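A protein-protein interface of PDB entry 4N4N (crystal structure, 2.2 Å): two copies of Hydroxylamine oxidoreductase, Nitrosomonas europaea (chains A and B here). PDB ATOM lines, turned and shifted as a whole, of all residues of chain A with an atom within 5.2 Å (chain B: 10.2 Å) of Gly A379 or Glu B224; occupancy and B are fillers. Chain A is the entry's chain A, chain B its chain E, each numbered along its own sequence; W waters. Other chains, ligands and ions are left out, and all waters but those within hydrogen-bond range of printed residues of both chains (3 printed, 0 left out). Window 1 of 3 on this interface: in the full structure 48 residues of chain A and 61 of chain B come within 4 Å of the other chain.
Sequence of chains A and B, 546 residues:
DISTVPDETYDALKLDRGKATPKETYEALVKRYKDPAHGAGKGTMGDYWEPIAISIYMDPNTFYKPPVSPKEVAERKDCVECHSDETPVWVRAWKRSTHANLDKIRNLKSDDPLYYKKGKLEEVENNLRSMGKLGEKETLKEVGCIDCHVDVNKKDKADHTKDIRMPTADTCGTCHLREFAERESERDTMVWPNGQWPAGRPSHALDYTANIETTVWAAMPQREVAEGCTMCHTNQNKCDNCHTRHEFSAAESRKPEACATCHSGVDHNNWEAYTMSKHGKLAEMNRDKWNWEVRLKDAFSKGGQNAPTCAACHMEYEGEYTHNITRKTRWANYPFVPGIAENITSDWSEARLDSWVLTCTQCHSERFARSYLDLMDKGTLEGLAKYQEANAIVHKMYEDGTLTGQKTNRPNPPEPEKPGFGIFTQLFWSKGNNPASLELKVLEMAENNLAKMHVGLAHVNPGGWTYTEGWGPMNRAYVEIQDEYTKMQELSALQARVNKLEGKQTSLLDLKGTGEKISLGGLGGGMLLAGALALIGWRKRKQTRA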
ATOM      1  N   ASP A 374       1.109  14.002  29.900  1.00  0.00           N
ATOM      2  CA  ASP A 374      -0.039  13.357  29.258  1.00  0.00           C
ATOM      3  C   ASP A 374      -0.503  14.176  28.054  1.00  0.00           C
ATOM      4  O   ASP A 374      -0.817  13.621  26.998  1.00  0.00           O
ATOM      5  CB  ASP A 374      -1.188  13.194  30.255  1.00  0.00           C
ATOM      6  CG  ASP A 374      -2.400  12.528  29.640  1.00  0.00           C
ATOM      7  OD1 ASP A 374      -3.395  13.234  29.370  1.00  0.00           O
ATOM      8  OD2 ASP A 374      -2.352  11.301  29.412  1.00  0.00           O
ATOM      9  N   LEU A 375      -0.541  15.496  28.233  1.00  0.00           N
ATOM     10  CA  LEU A 375      -0.852  16.430  27.158  1.00  0.00           C
ATOM     11  C   LEU A 375       0.155  16.269  26.016  1.00  0.00           C
ATOM     12  O   LEU A 375      -0.238  16.185  24.848  1.00  0.00           O
ATOM     13  CB  LEU A 375      -0.864  17.875  27.690  1.00  0.00           C
ATOM     14  CG  LEU A 375      -1.340  19.060  26.835  1.00  0.00           C
ATOM     15  CD1 LEU A 375      -1.613  20.274  27.705  1.00  0.00           C
ATOM     16  CD2 LEU A 375      -0.348  19.429  25.743  1.00  0.00           C
ATOM     17  N   MET A 376       1.440  16.214  26.365  1.00  0.00           N
ATOM     18  CA  MET A 376       2.521  16.081  25.384  1.00  0.00           C
ATOM     19  C   MET A 376       2.365  14.817  24.539  1.00  0.00           C
ATOM     20  O   MET A 376       2.462  14.872  23.310  1.00  0.00           O
ATOM     21  CB  MET A 376       3.889  16.099  26.080  1.00  0.00           C
ATOM     22  CG  MET A 376       5.086  15.820  25.161  1.00  0.00           C
ATOM     23  SD  MET A 376       6.577  15.296  26.048  1.00  0.00           S
ATOM     24  CE  MET A 376       6.101  13.644  26.568  1.00  0.00           C
ATOM     25  N   ASP A 377       2.112  13.690  25.209  1.00  0.00           N
ATOM     26  CA  ASP A 377       1.939  12.405  24.537  1.00  0.00           C
ATOM     27  C   ASP A 377       0.753  12.422  23.583  1.00  0.00           C
ATOM     28  O   ASP A 377       0.874  11.993  22.438  1.00  0.00           O
ATOM     29  CB  ASP A 377       1.794  11.262  25.553  1.00  0.00           C
ATOM     30  CG  ASP A 377       3.124  10.850  26.176  1.00  0.00           C
ATOM     31  OD1 ASP A 377       4.194  11.155  25.598  1.00  0.00           O
ATOM     32  OD2 ASP A 377       3.096  10.213  27.252  1.00  0.00           O
ATOM     33  N   LYS A 378      -0.379  12.943  24.051  1.00  0.00           N
ATOM     34  CA  LYS A 378      -1.613  12.942  23.262  1.00  0.00           C
ATOM     35  C   LYS A 378      -1.619  13.985  22.151  1.00  0.00           C
ATOM     36  O   LYS A 378      -2.113  13.723  21.056  1.00  0.00           O
ATOM     37  CB  LYS A 378      -2.839  13.095  24.162  1.00  0.00           C
ATOM     38  CG  LYS A 378      -3.225  11.812  24.865  1.00  0.00           C
ATOM     39  CD  LYS A 378      -4.272  12.053  25.933  1.00  0.00           C
ATOM     40  CE  LYS A 378      -4.474  10.808  26.779  1.00  0.00           C
ATOM     41  NZ  LYS A 378      -5.109  11.148  28.079  1.00  0.00           N
ATOM     42  N   GLY A 379      -1.068  15.163  22.434  1.00  0.00           N
ATOM     43  CA  GLY A 379      -0.893  16.192  21.410  1.00  0.00           C
ATOM     44  C   GLY A 379      -0.034  15.686  20.267  1.00  0.00           C
ATOM     45  O   GLY A 379      -0.312  15.962  19.102  1.00  0.00           O
ATOM     46  N   THR A 380       1.010  14.934  20.615  1.00  0.00           N
ATOM     47  CA  THR A 380       1.922  14.339  19.639  1.00  0.00           C
ATOM     48  C   THR A 380       1.196  13.338  18.736  1.00  0.00           C
ATOM     49  O   THR A 380       1.343  13.380  17.509  1.00  0.00           O
ATOM     50  CB  THR A 380       3.124  13.672  20.345  1.00  0.00           C
ATOM     51  OG1 THR A 380       3.826  14.656  21.119  1.00  0.00           O
ATOM     52  CG2 THR A 380       4.087  13.050  19.342  1.00  0.00           C
ATOM     53  N   LEU A 381       0.401  12.455  19.342  1.00  0.00           N
ATOM     54  CA  LEU A 381      -0.379  11.475  18.585  1.00  0.00           C
ATOM     55  C   LEU A 381      -1.428  12.143  17.682  1.00  0.00           C
ATOM     56  O   LEU A 381      -1.689  11.671  16.567  1.00  0.00           O
ATOM     57  CB  LEU A 381      -1.039  10.462  19.527  1.00  0.00           C
ATOM     58  CG  LEU A 381      -0.145   9.474  20.292  1.00  0.00           C
ATOM     59  CD1 LEU A 381      -0.874   8.920  21.508  1.00  0.00           C
ATOM     60  CD2 LEU A 381       0.347   8.338  19.393  1.00  0.00           C
ATOM     61  N   GLU A 382      -2.016  13.239  18.164  1.00  0.00           N
ATOM     62  CA  GLU A 382      -2.986  14.012  17.376  1.00  0.00           C
ATOM     63  C   GLU A 382      -2.356  14.600  16.109  1.00  0.00           C
ATOM     64  O   GLU A 382      -2.979  14.622  15.049  1.00  0.00           O
ATOM     65  CB  GLU A 382      -3.629  15.111  18.232  1.00  0.00           C
ATOM     66  CG  GLU A 382      -4.701  14.589  19.179  1.00  0.00           C
ATOM     67  CD  GLU A 382      -4.838  15.403  20.458  1.00  0.00           C
ATOM     68  OE1 GLU A 382      -4.423  16.584  20.494  1.00  0.00           O
ATOM     69  OE2 GLU A 382      -5.375  14.850  21.439  1.00  0.00           O
ATOM     70  N   GLY A 383      -1.118  15.073  16.230  1.00  0.00           N
ATOM     71  CA  GLY A 383      -0.347  15.523  15.079  1.00  0.00           C
ATOM     72  C   GLY A 383      -0.019  14.377  14.133  1.00  0.00           C
ATOM     73  O   GLY A 383      -0.138  14.523  12.911  1.00  0.00           O
ATOM     74  N   MET A 453       6.203  20.077  16.024  1.00  0.00           N
ATOM     75  CA  MET A 453       5.024  20.003  16.891  1.00  0.00           C
ATOM     76  C   MET A 453       5.340  19.274  18.193  1.00  0.00           C
ATOM     77  O   MET A 453       5.044  19.780  19.279  1.00  0.00           O
ATOM     78  CB  MET A 453       3.854  19.303  16.189  1.00  0.00           C
ATOM     79  CG  MET A 453       2.566  19.327  17.007  1.00  0.00           C
ATOM     80  SD  MET A 453       1.144  18.636  16.145  1.00  0.00           S
ATOM     81  CE  MET A 453      -0.099  18.765  17.423  1.00  0.00           C
ATOM     82  N   LEU A 457       5.595  20.741  22.101  1.00  0.00           N
ATOM     83  CA  LEU A 457       4.906  20.086  23.214  1.00  0.00           C
ATOM     84  C   LEU A 457       5.876  19.657  24.308  1.00  0.00           C
ATOM     85  O   LEU A 457       5.654  19.954  25.484  1.00  0.00           O
ATOM     86  CB  LEU A 457       4.104  18.873  22.724  1.00  0.00           C
ATOM     87  CG  LEU A 457       2.804  19.156  21.966  1.00  0.00           C
ATOM     88  CD1 LEU A 457       2.462  18.021  21.012  1.00  0.00           C
ATOM     89  CD2 LEU A 457       1.655  19.407  22.932  1.00  0.00           C
ATOM     90  N   TRP A 465       3.238  24.340  19.013  1.00  0.00           N
ATOM     91  CA  TRP A 465       2.450  23.193  18.568  1.00  0.00           C
ATOM     92  C   TRP A 465       1.075  23.588  18.048  1.00  0.00           C
ATOM     93  O   TRP A 465       0.327  22.742  17.576  1.00  0.00           O
ATOM     94  CB  TRP A 465       2.390  22.080  19.631  1.00  0.00           C
ATOM     95  CG  TRP A 465       1.448  22.281  20.794  1.00  0.00           C
ATOM     96  CD1 TRP A 465       0.096  22.050  20.808  1.00  0.00           C
ATOM     97  CD2 TRP A 465       1.796  22.689  22.126  1.00  0.00           C
ATOM     98  NE1 TRP A 465      -0.418  22.308  22.058  1.00  0.00           N
ATOM     99  CE2 TRP A 465       0.601  22.702  22.885  1.00  0.00           C
ATOM    100  CE3 TRP A 465       2.998  23.046  22.751  1.00  0.00           C
ATOM    101  CZ2 TRP A 465       0.577  23.057  24.241  1.00  0.00           C
ATOM    102  CZ3 TRP A 465       2.975  23.404  24.093  1.00  0.00           C
ATOM    103  CH2 TRP A 465       1.769  23.411  24.824  1.00  0.00           C
ATOM    104  N   TRP B  49     -17.114  20.431  25.069  1.00  0.00           N
ATOM    105  CA  TRP B  49     -15.754  20.077  25.464  1.00  0.00           C
ATOM    106  C   TRP B  49     -15.664  19.700  26.934  1.00  0.00           C
ATOM    107  O   TRP B  49     -16.454  20.163  27.754  1.00  0.00           O
ATOM    108  CB  TRP B  49     -14.779  21.225  25.161  1.00  0.00           C
ATOM    109  CG  TRP B  49     -15.082  22.495  25.910  1.00  0.00           C
ATOM    110  CD1 TRP B  49     -15.934  23.485  25.524  1.00  0.00           C
ATOM    111  CD2 TRP B  49     -14.531  22.909  27.170  1.00  0.00           C
ATOM    112  NE1 TRP B  49     -15.951  24.490  26.459  1.00  0.00           N
ATOM    113  CE2 TRP B  49     -15.103  24.161  27.482  1.00  0.00           C
ATOM    114  CE3 TRP B  49     -13.610  22.343  28.064  1.00  0.00           C
ATOM    115  CZ2 TRP B  49     -14.782  24.865  28.649  1.00  0.00           C
ATOM    116  CZ3 TRP B  49     -13.294  23.041  29.229  1.00  0.00           C
ATOM    117  CH2 TRP B  49     -13.877  24.291  29.509  1.00  0.00           C
ATOM    118  N   GLU B  50     -14.685  18.858  27.247  1.00  0.00           N
ATOM    119  CA  GLU B  50     -14.420  18.426  28.612  1.00  0.00           C
ATOM    120  C   GLU B  50     -13.004  18.837  28.987  1.00  0.00           C
ATOM    121  O   GLU B  50     -12.125  18.878  28.123  1.00  0.00           O
ATOM    122  CB  GLU B  50     -14.579  16.902  28.741  1.00  0.00           C
ATOM    123  CG  GLU B  50     -16.029  16.403  28.731  1.00  0.00           C
ATOM    124  CD  GLU B  50     -16.712  16.588  27.388  1.00  0.00           C
ATOM    125  OE1 GLU B  50     -17.858  17.088  27.360  1.00  0.00           O
ATOM    126  OE2 GLU B  50     -16.095  16.257  26.353  1.00  0.00           O
ATOM    127  N   PRO B  51     -12.773  19.149  30.273  1.00  0.00           N
ATOM    128  CA  PRO B  51     -11.419  19.480  30.707  1.00  0.00           C
ATOM    129  C   PRO B  51     -10.482  18.283  30.571  1.00  0.00           C
ATOM    130  O   PRO B  51     -10.925  17.133  30.650  1.00  0.00           O
ATOM    131  CB  PRO B  51     -11.606  19.833  32.186  1.00  0.00           C
ATOM    132  CG  PRO B  51     -12.855  19.111  32.595  1.00  0.00           C
ATOM    133  CD  PRO B  51     -13.734  19.191  31.391  1.00  0.00           C
ATOM    134  N   ILE B  52      -9.203  18.557  30.342  1.00  0.00           N
ATOM    135  CA  ILE B  52      -8.169  17.532  30.433  1.00  0.00           C
ATOM    136  C   ILE B  52      -7.450  17.713  31.769  1.00  0.00           C
ATOM    137  O   ILE B  52      -7.816  18.593  32.551  1.00  0.00           O
ATOM    138  CB  ILE B  52      -7.201  17.549  29.215  1.00  0.00           C
ATOM    139  CG1 ILE B  52      -6.527  18.920  29.051  1.00  0.00           C
ATOM    140  CG2 ILE B  52      -7.952  17.151  27.945  1.00  0.00           C
ATOM    141  CD1 ILE B  52      -5.476  18.973  27.937  1.00  0.00           C
ATOM    142  N   ALA B  53      -6.448  16.883  32.041  1.00  0.00           N
ATOM    143  CA  ALA B  53      -5.768  16.895  33.337  1.00  0.00           C
ATOM    144  C   ALA B  53      -5.176  18.261  33.707  1.00  0.00           C
ATOM    145  O   ALA B  53      -5.292  18.701  34.852  1.00  0.00           O
ATOM    146  CB  ALA B  53      -4.699  15.807  33.388  1.00  0.00           C
ATOM    147  N   ILE B  54      -4.559  18.930  32.733  1.00  0.00           N
ATOM    148  CA  ILE B  54      -3.901  20.219  32.963  1.00  0.00           C
ATOM    149  C   ILE B  54      -4.906  21.361  33.202  1.00  0.00           C
ATOM    150  O   ILE B  54      -4.532  22.432  33.692  1.00  0.00           O
ATOM    151  CB  ILE B  54      -2.918  20.576  31.804  1.00  0.00           C
ATOM    152  CG1 ILE B  54      -1.839  21.567  32.267  1.00  0.00           C
ATOM    153  CG2 ILE B  54      -3.664  21.111  30.585  1.00  0.00           C
ATOM    154  CD1 ILE B  54      -0.677  20.932  33.018  1.00  0.00           C
ATOM    155  N   SER B  55      -6.175  21.118  32.872  1.00  0.00           N
ATOM    156  CA  SER B  55      -7.224  22.145  32.970  1.00  0.00           C
ATOM    157  C   SER B  55      -7.513  22.605  34.392  1.00  0.00           C
ATOM    158  O   SER B  55      -8.049  23.694  34.584  1.00  0.00           O
ATOM    159  CB  SER B  55      -8.521  21.676  32.313  1.00  0.00           C
ATOM    160  OG  SER B  55      -8.324  21.398  30.941  1.00  0.00           O
ATOM    161  N   MET B  58      -5.308  25.558  34.711  1.00  0.00           N
ATOM    162  CA  MET B  58      -5.655  26.633  33.775  1.00  0.00           C
ATOM    163  C   MET B  58      -6.909  27.394  34.208  1.00  0.00           C
ATOM    164  O   MET B  58      -6.947  28.627  34.131  1.00  0.00           O
ATOM    165  CB  MET B  58      -5.845  26.080  32.359  1.00  0.00           C
ATOM    166  CG  MET B  58      -4.663  25.282  31.815  1.00  0.00           C
ATOM    167  SD  MET B  58      -3.204  26.271  31.414  1.00  0.00           S
ATOM    168  CE  MET B  58      -2.221  26.096  32.902  1.00  0.00           C
ATOM    169  N   VAL B 216     -13.773  27.015  17.246  1.00  0.00           N
ATOM    170  CA  VAL B 216     -12.921  25.822  17.033  1.00  0.00           C
ATOM    171  C   VAL B 216     -12.326  25.274  18.309  1.00  0.00           C
ATOM    172  O   VAL B 216     -12.144  24.066  18.430  1.00  0.00           O
ATOM    173  CB  VAL B 216     -11.702  26.014  16.096  1.00  0.00           C
ATOM    174  CG1 VAL B 216     -11.884  25.240  14.811  1.00  0.00           C
ATOM    175  CG2 VAL B 216     -11.326  27.466  15.905  1.00  0.00           C
ATOM    176  N   TRP B 217     -11.988  26.165  19.237  1.00  0.00           N
ATOM    177  CA  TRP B 217     -11.399  25.745  20.499  1.00  0.00           C
ATOM    178  C   TRP B 217     -12.335  24.769  21.202  1.00  0.00           C
ATOM    179  O   TRP B 217     -11.896  23.744  21.723  1.00  0.00           O
ATOM    180  CB  TRP B 217     -11.093  26.944  21.394  1.00  0.00           C
ATOM    181  CG  TRP B 217     -10.448  26.536  22.679  1.00  0.00           C
ATOM    182  CD1 TRP B 217      -9.113  26.453  22.936  1.00  0.00           C
ATOM    183  CD2 TRP B 217     -11.118  26.130  23.880  1.00  0.00           C
ATOM    184  NE1 TRP B 217      -8.905  26.028  24.229  1.00  0.00           N
ATOM    185  CE2 TRP B 217     -10.120  25.821  24.829  1.00  0.00           C
ATOM    186  CE3 TRP B 217     -12.465  26.002  24.247  1.00  0.00           C
ATOM    187  CZ2 TRP B 217     -10.426  25.391  26.123  1.00  0.00           C
ATOM    188  CZ3 TRP B 217     -12.768  25.577  25.529  1.00  0.00           C
ATOM    189  CH2 TRP B 217     -11.752  25.275  26.453  1.00  0.00           C
ATOM    190  N   MET B 220     -13.234  21.524  18.159  1.00  0.00           N
ATOM    191  CA  MET B 220     -12.220  20.583  17.650  1.00  0.00           C
ATOM    192  C   MET B 220     -11.985  19.405  18.601  1.00  0.00           C
ATOM    193  O   MET B 220     -12.012  19.583  19.817  1.00  0.00           O
ATOM    194  CB  MET B 220     -10.903  21.301  17.336  1.00  0.00           C
ATOM    195  CG  MET B 220     -10.123  21.791  18.554  1.00  0.00           C
ATOM    196  SD  MET B 220      -8.826  22.969  18.131  1.00  0.00           S
ATOM    197  CE  MET B 220      -7.553  21.887  17.475  1.00  0.00           C
ATOM    198  N   PRO B 221     -11.762  18.196  18.042  1.00  0.00           N
ATOM    199  CA  PRO B 221     -11.534  16.999  18.861  1.00  0.00           C
ATOM    200  C   PRO B 221     -10.156  16.952  19.522  1.00  0.00           C
ATOM    201  O   PRO B 221      -9.997  16.315  20.567  1.00  0.00           O
ATOM    202  CB  PRO B 221     -11.684  15.853  17.856  1.00  0.00           C
ATOM    203  CG  PRO B 221     -11.359  16.460  16.536  1.00  0.00           C
ATOM    204  CD  PRO B 221     -11.868  17.867  16.606  1.00  0.00           C
ATOM    205  N   GLN B 222      -9.179  17.631  18.923  1.00  0.00           N
ATOM    206  CA  GLN B 222      -7.807  17.629  19.429  1.00  0.00           C
ATOM    207  C   GLN B 222      -7.691  18.544  20.649  1.00  0.00           C
ATOM    208  O   GLN B 222      -7.279  19.703  20.532  1.00  0.00           O
ATOM    209  CB  GLN B 222      -6.815  18.049  18.333  1.00  0.00           C
ATOM    210  CG  GLN B 222      -6.815  17.173  17.078  1.00  0.00           C
ATOM    211  CD  GLN B 222      -7.891  17.559  16.070  1.00  0.00           C
ATOM    212  OE1 GLN B 222      -8.670  18.488  16.294  1.00  0.00           O
ATOM    213  NE2 GLN B 222      -7.933  16.846  14.945  1.00  0.00           N
ATOM    214  N   ARG B 223      -8.051  18.012  21.815  1.00  0.00           N
ATOM    215  CA  ARG B 223      -8.109  18.811  23.047  1.00  0.00           C
ATOM    216  C   ARG B 223      -6.745  19.339  23.491  1.00  0.00           C
ATOM    217  O   ARG B 223      -6.632  20.477  23.964  1.00  0.00           O
ATOM    218  CB  ARG B 223      -8.763  18.020  24.191  1.00  0.00           C
ATOM    219  CG  ARG B 223     -10.233  17.633  23.961  1.00  0.00           C
ATOM    220  CD  ARG B 223     -11.071  18.789  23.416  1.00  0.00           C
ATOM    221  NE  ARG B 223     -10.915  20.031  24.181  1.00  0.00           N
ATOM    222  CZ  ARG B 223     -11.267  21.230  23.727  1.00  0.00           C
ATOM    223  NH1 ARG B 223     -11.798  21.354  22.517  1.00  0.00           N
ATOM    224  NH2 ARG B 223     -11.090  22.307  24.479  1.00  0.00           N
ATOM    225  N   GLU B 224      -5.722  18.502  23.339  1.00  0.00           N
ATOM    226  CA  GLU B 224      -4.372  18.849  23.760  1.00  0.00           C
ATOM    227  C   GLU B 224      -3.775  19.953  22.878  1.00  0.00           C
ATOM    228  O   GLU B 224      -2.947  20.740  23.340  1.00  0.00           O
ATOM    229  CB  GLU B 224      -3.483  17.597  23.793  1.00  0.00           C
ATOM    230  CG  GLU B 224      -3.733  16.672  25.006  1.00  0.00           C
ATOM    231  CD  GLU B 224      -5.066  15.904  24.965  1.00  0.00           C
ATOM    232  OE1 GLU B 224      -5.686  15.783  23.885  1.00  0.00           O
ATOM    233  OE2 GLU B 224      -5.493  15.408  26.031  1.00  0.00           O
ATOM    234  N   VAL B 225      -4.215  20.018  21.622  1.00  0.00           N
ATOM    235  CA  VAL B 225      -3.851  21.124  20.729  1.00  0.00           C
ATOM    236  C   VAL B 225      -4.550  22.409  21.184  1.00  0.00           C
ATOM    237  O   VAL B 225      -3.898  23.435  21.392  1.00  0.00           O
ATOM    238  CB  VAL B 225      -4.196  20.827  19.245  1.00  0.00           C
ATOM    239  CG1 VAL B 225      -3.857  22.022  18.359  1.00  0.00           C
ATOM    240  CG2 VAL B 225      -3.467  19.578  18.760  1.00  0.00           C
ATOM    241  N   ALA B 226      -5.872  22.339  21.346  1.00  0.00           N
ATOM    242  CA  ALA B 226      -6.673  23.477  21.809  1.00  0.00           C
ATOM    243  C   ALA B 226      -6.146  24.083  23.108  1.00  0.00           C
ATOM    244  O   ALA B 226      -6.181  25.298  23.286  1.00  0.00           O
ATOM    245  CB  ALA B 226      -8.135  23.075  21.965  1.00  0.00           C
ATOM    246  N   GLU B 227      -5.644  23.232  24.001  1.00  0.00           N
ATOM    247  CA  GLU B 227      -5.196  23.658  25.328  1.00  0.00           C
ATOM    248  C   GLU B 227      -3.854  24.414  25.306  1.00  0.00           C
ATOM    249  O   GLU B 227      -3.489  25.076  26.281  1.00  0.00           O
ATOM    250  CB  GLU B 227      -5.141  22.460  26.284  1.00  0.00           C
ATOM    251  CG  GLU B 227      -5.275  22.820  27.776  1.00  0.00           C
ATOM    252  CD  GLU B 227      -6.678  23.300  28.185  1.00  0.00           C
ATOM    253  OE1 GLU B 227      -7.582  23.387  27.325  1.00  0.00           O
ATOM    254  OE2 GLU B 227      -6.873  23.587  29.388  1.00  0.00           O
ATOM    255  N   GLY B 228      -3.131  24.302  24.196  1.00  0.00           N
ATOM    256  CA  GLY B 228      -1.981  25.159  23.935  1.00  0.00           C
ATOM    257  C   GLY B 228      -2.414  26.610  23.822  1.00  0.00           C
ATOM    258  O   GLY B 228      -1.722  27.511  24.298  1.00  0.00           O
ATOM    259  N   CYS B 229      -3.570  26.829  23.196  1.00  0.00           N
ATOM    260  CA  CYS B 229      -4.171  28.158  23.113  1.00  0.00           C
ATOM    261  C   CYS B 229      -4.512  28.673  24.505  1.00  0.00           C
ATOM    262  O   CYS B 229      -4.238  29.826  24.828  1.00  0.00           O
ATOM    263  CB  CYS B 229      -5.432  28.130  22.247  1.00  0.00           C
ATOM    264  SG  CYS B 229      -5.204  27.354  20.646  1.00  0.00           S
ATOM    265  N   THR B 230      -5.096  27.800  25.324  1.00  0.00           N
ATOM    266  CA  THR B 230      -5.446  28.105  26.709  1.00  0.00           C
ATOM    267  C   THR B 230      -4.241  28.623  27.510  1.00  0.00           C
ATOM    268  O   THR B 230      -4.366  29.580  28.275  1.00  0.00           O
ATOM    269  CB  THR B 230      -6.067  26.865  27.410  1.00  0.00           C
ATOM    270  OG1 THR B 230      -7.184  26.385  26.646  1.00  0.00           O
ATOM    271  CG2 THR B 230      -6.534  27.203  28.821  1.00  0.00           C
ATOM    272  N   MET B 231      -3.083  27.997  27.321  1.00  0.00           N
ATOM    273  CA  MET B 231      -1.865  28.363  28.055  1.00  0.00           C
ATOM    274  C   MET B 231      -1.412  29.817  27.830  1.00  0.00           C
ATOM    275  O   MET B 231      -0.801  30.419  28.711  1.00  0.00           O
ATOM    276  CB  MET B 231      -0.739  27.365  27.758  1.00  0.00           C
ATOM    277  CG  MET B 231      -0.996  25.972  28.358  1.00  0.00           C
ATOM    278  SD  MET B 231       0.312  24.746  28.108  1.00  0.00           S
ATOM    279  CE  MET B 231       1.694  25.535  28.922  1.00  0.00           C
ATOM    280  N   PHE B 428      -7.564  25.843  12.444  1.00  0.00           N
ATOM    281  CA  PHE B 428      -7.389  24.791  13.450  1.00  0.00           C
ATOM    282  C   PHE B 428      -8.142  23.494  13.145  1.00  0.00           C
ATOM    283  O   PHE B 428      -8.017  22.510  13.878  1.00  0.00           O
ATOM    284  CB  PHE B 428      -7.729  25.327  14.847  1.00  0.00           C
ATOM    285  CG  PHE B 428      -6.647  26.185  15.426  1.00  0.00           C
ATOM    286  CD1 PHE B 428      -5.650  25.626  16.220  1.00  0.00           C
ATOM    287  CD2 PHE B 428      -6.594  27.544  15.141  1.00  0.00           C
ATOM    288  CE1 PHE B 428      -4.625  26.412  16.740  1.00  0.00           C
ATOM    289  CE2 PHE B 428      -5.573  28.342  15.653  1.00  0.00           C
ATOM    290  CZ  PHE B 428      -4.587  27.774  16.455  1.00  0.00           C
HETATM  291  O   HOH W   1      -6.047  14.505  30.338  1.00  0.00           O
HETATM  292  O   HOH W   2      -5.572  14.860  14.309  1.00  0.00           O
HETATM  293  O   HOH W   3      -4.231  15.590  28.302  1.00  0.00           O
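No position is printed for both chains.
Of chain B, only Glu B224 comes within 4 Å of Gly A379.
Glu B224 touches just these residues of chain A: Leu A375, Lys A378, Gly A379, Glu A382 and Trp A465.
Of chain B, only Ile B54 and Glu B224 come within 4 Å of Leu A375.
Of the printed residues of chain A, Gly B228 touches Trp A465.
Of the printed residues of chain A, Ile B54 touches Leu A375.
Leu A381 touches none of the printed residues of chain B.
Val B216 touches none of the printed residues of chain A.
The nearest residue of chain B that does not touch Gly A379 is Val B225 (4.8 Å).
The nearest residue of chain A that does not touch Glu B224 is Asp A374 (4.5 Å).
The nearest printed residue of chain A that does not touch Gly B228 is Leu A375 (5.6 Å).
Of the 13 printed residues of chain A, 6 touch a printed residue of chain B.
Hydrophobic or aromatic side chains of chain A that line the printed part of chain B: Leu A375, Met A453 and Trp A465.
Of the 23 printed residues of chain B, 6 touch a printed residue of chain A.
Printed residues of chain B that touch a printed residue of chain A: Ile B54, Gln B222, Glu B224, Val B225, Gly B228 and Met B231.
Among the printed residues, no Asp or Glu carboxylate lies within 4 Å of a Lys or Arg side-chain nitrogen of the other chain.
OE2 of Glu A382 lies close to OE1 of Glu B224, at 2.6 Å.
The indole nitrogen (NE1) of Trp A465 sits at hydrogen-bond distance from the backbone carbonyl oxygen (O) of Glu B224, at 3.2 Å.
The side-chain amino group (NZ) of Lys A378 lies within salt-bridge range of the side-chain carboxylate (OD1) of Asp A374, 3.0 Å away.
Water W3 lies within hydrogen-bond range of the side-chain carboxylate of Glu B224 (2.6 Å) and the side-chain carboxylate of Asp A374 (2.7 Å).
Water W2 lies within hydrogen-bond range of the backbone carbonyl oxygen of Glu A382 and the side-chain amide nitrogen of Gln B222.
Water W1 lies within hydrogen-bond range of the backbone NH (N) of Ala B53 and the side-chain carboxylate (OD1) of Asp A374.
Among the printed residues, pairs that only touch across the chains: Leu A375 with Ile B54 (3.6 Å), Leu A375 with Glu B224 (3.5 Å), Lys A378 with Glu B224 (3.6 Å), Gly A379 with Glu B224 (3.7 Å), Glu A382 with Gln B222 (3.5 Å), Glu A382 with Val B225 (3.6 Å), Met A453 with Val B225 (3.7 Å), Trp A465 with Val B225 (3.7 Å), Trp A465 with Gly B228 (3.3 Å) and Trp A465 with Met B231 (3.8 Å).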
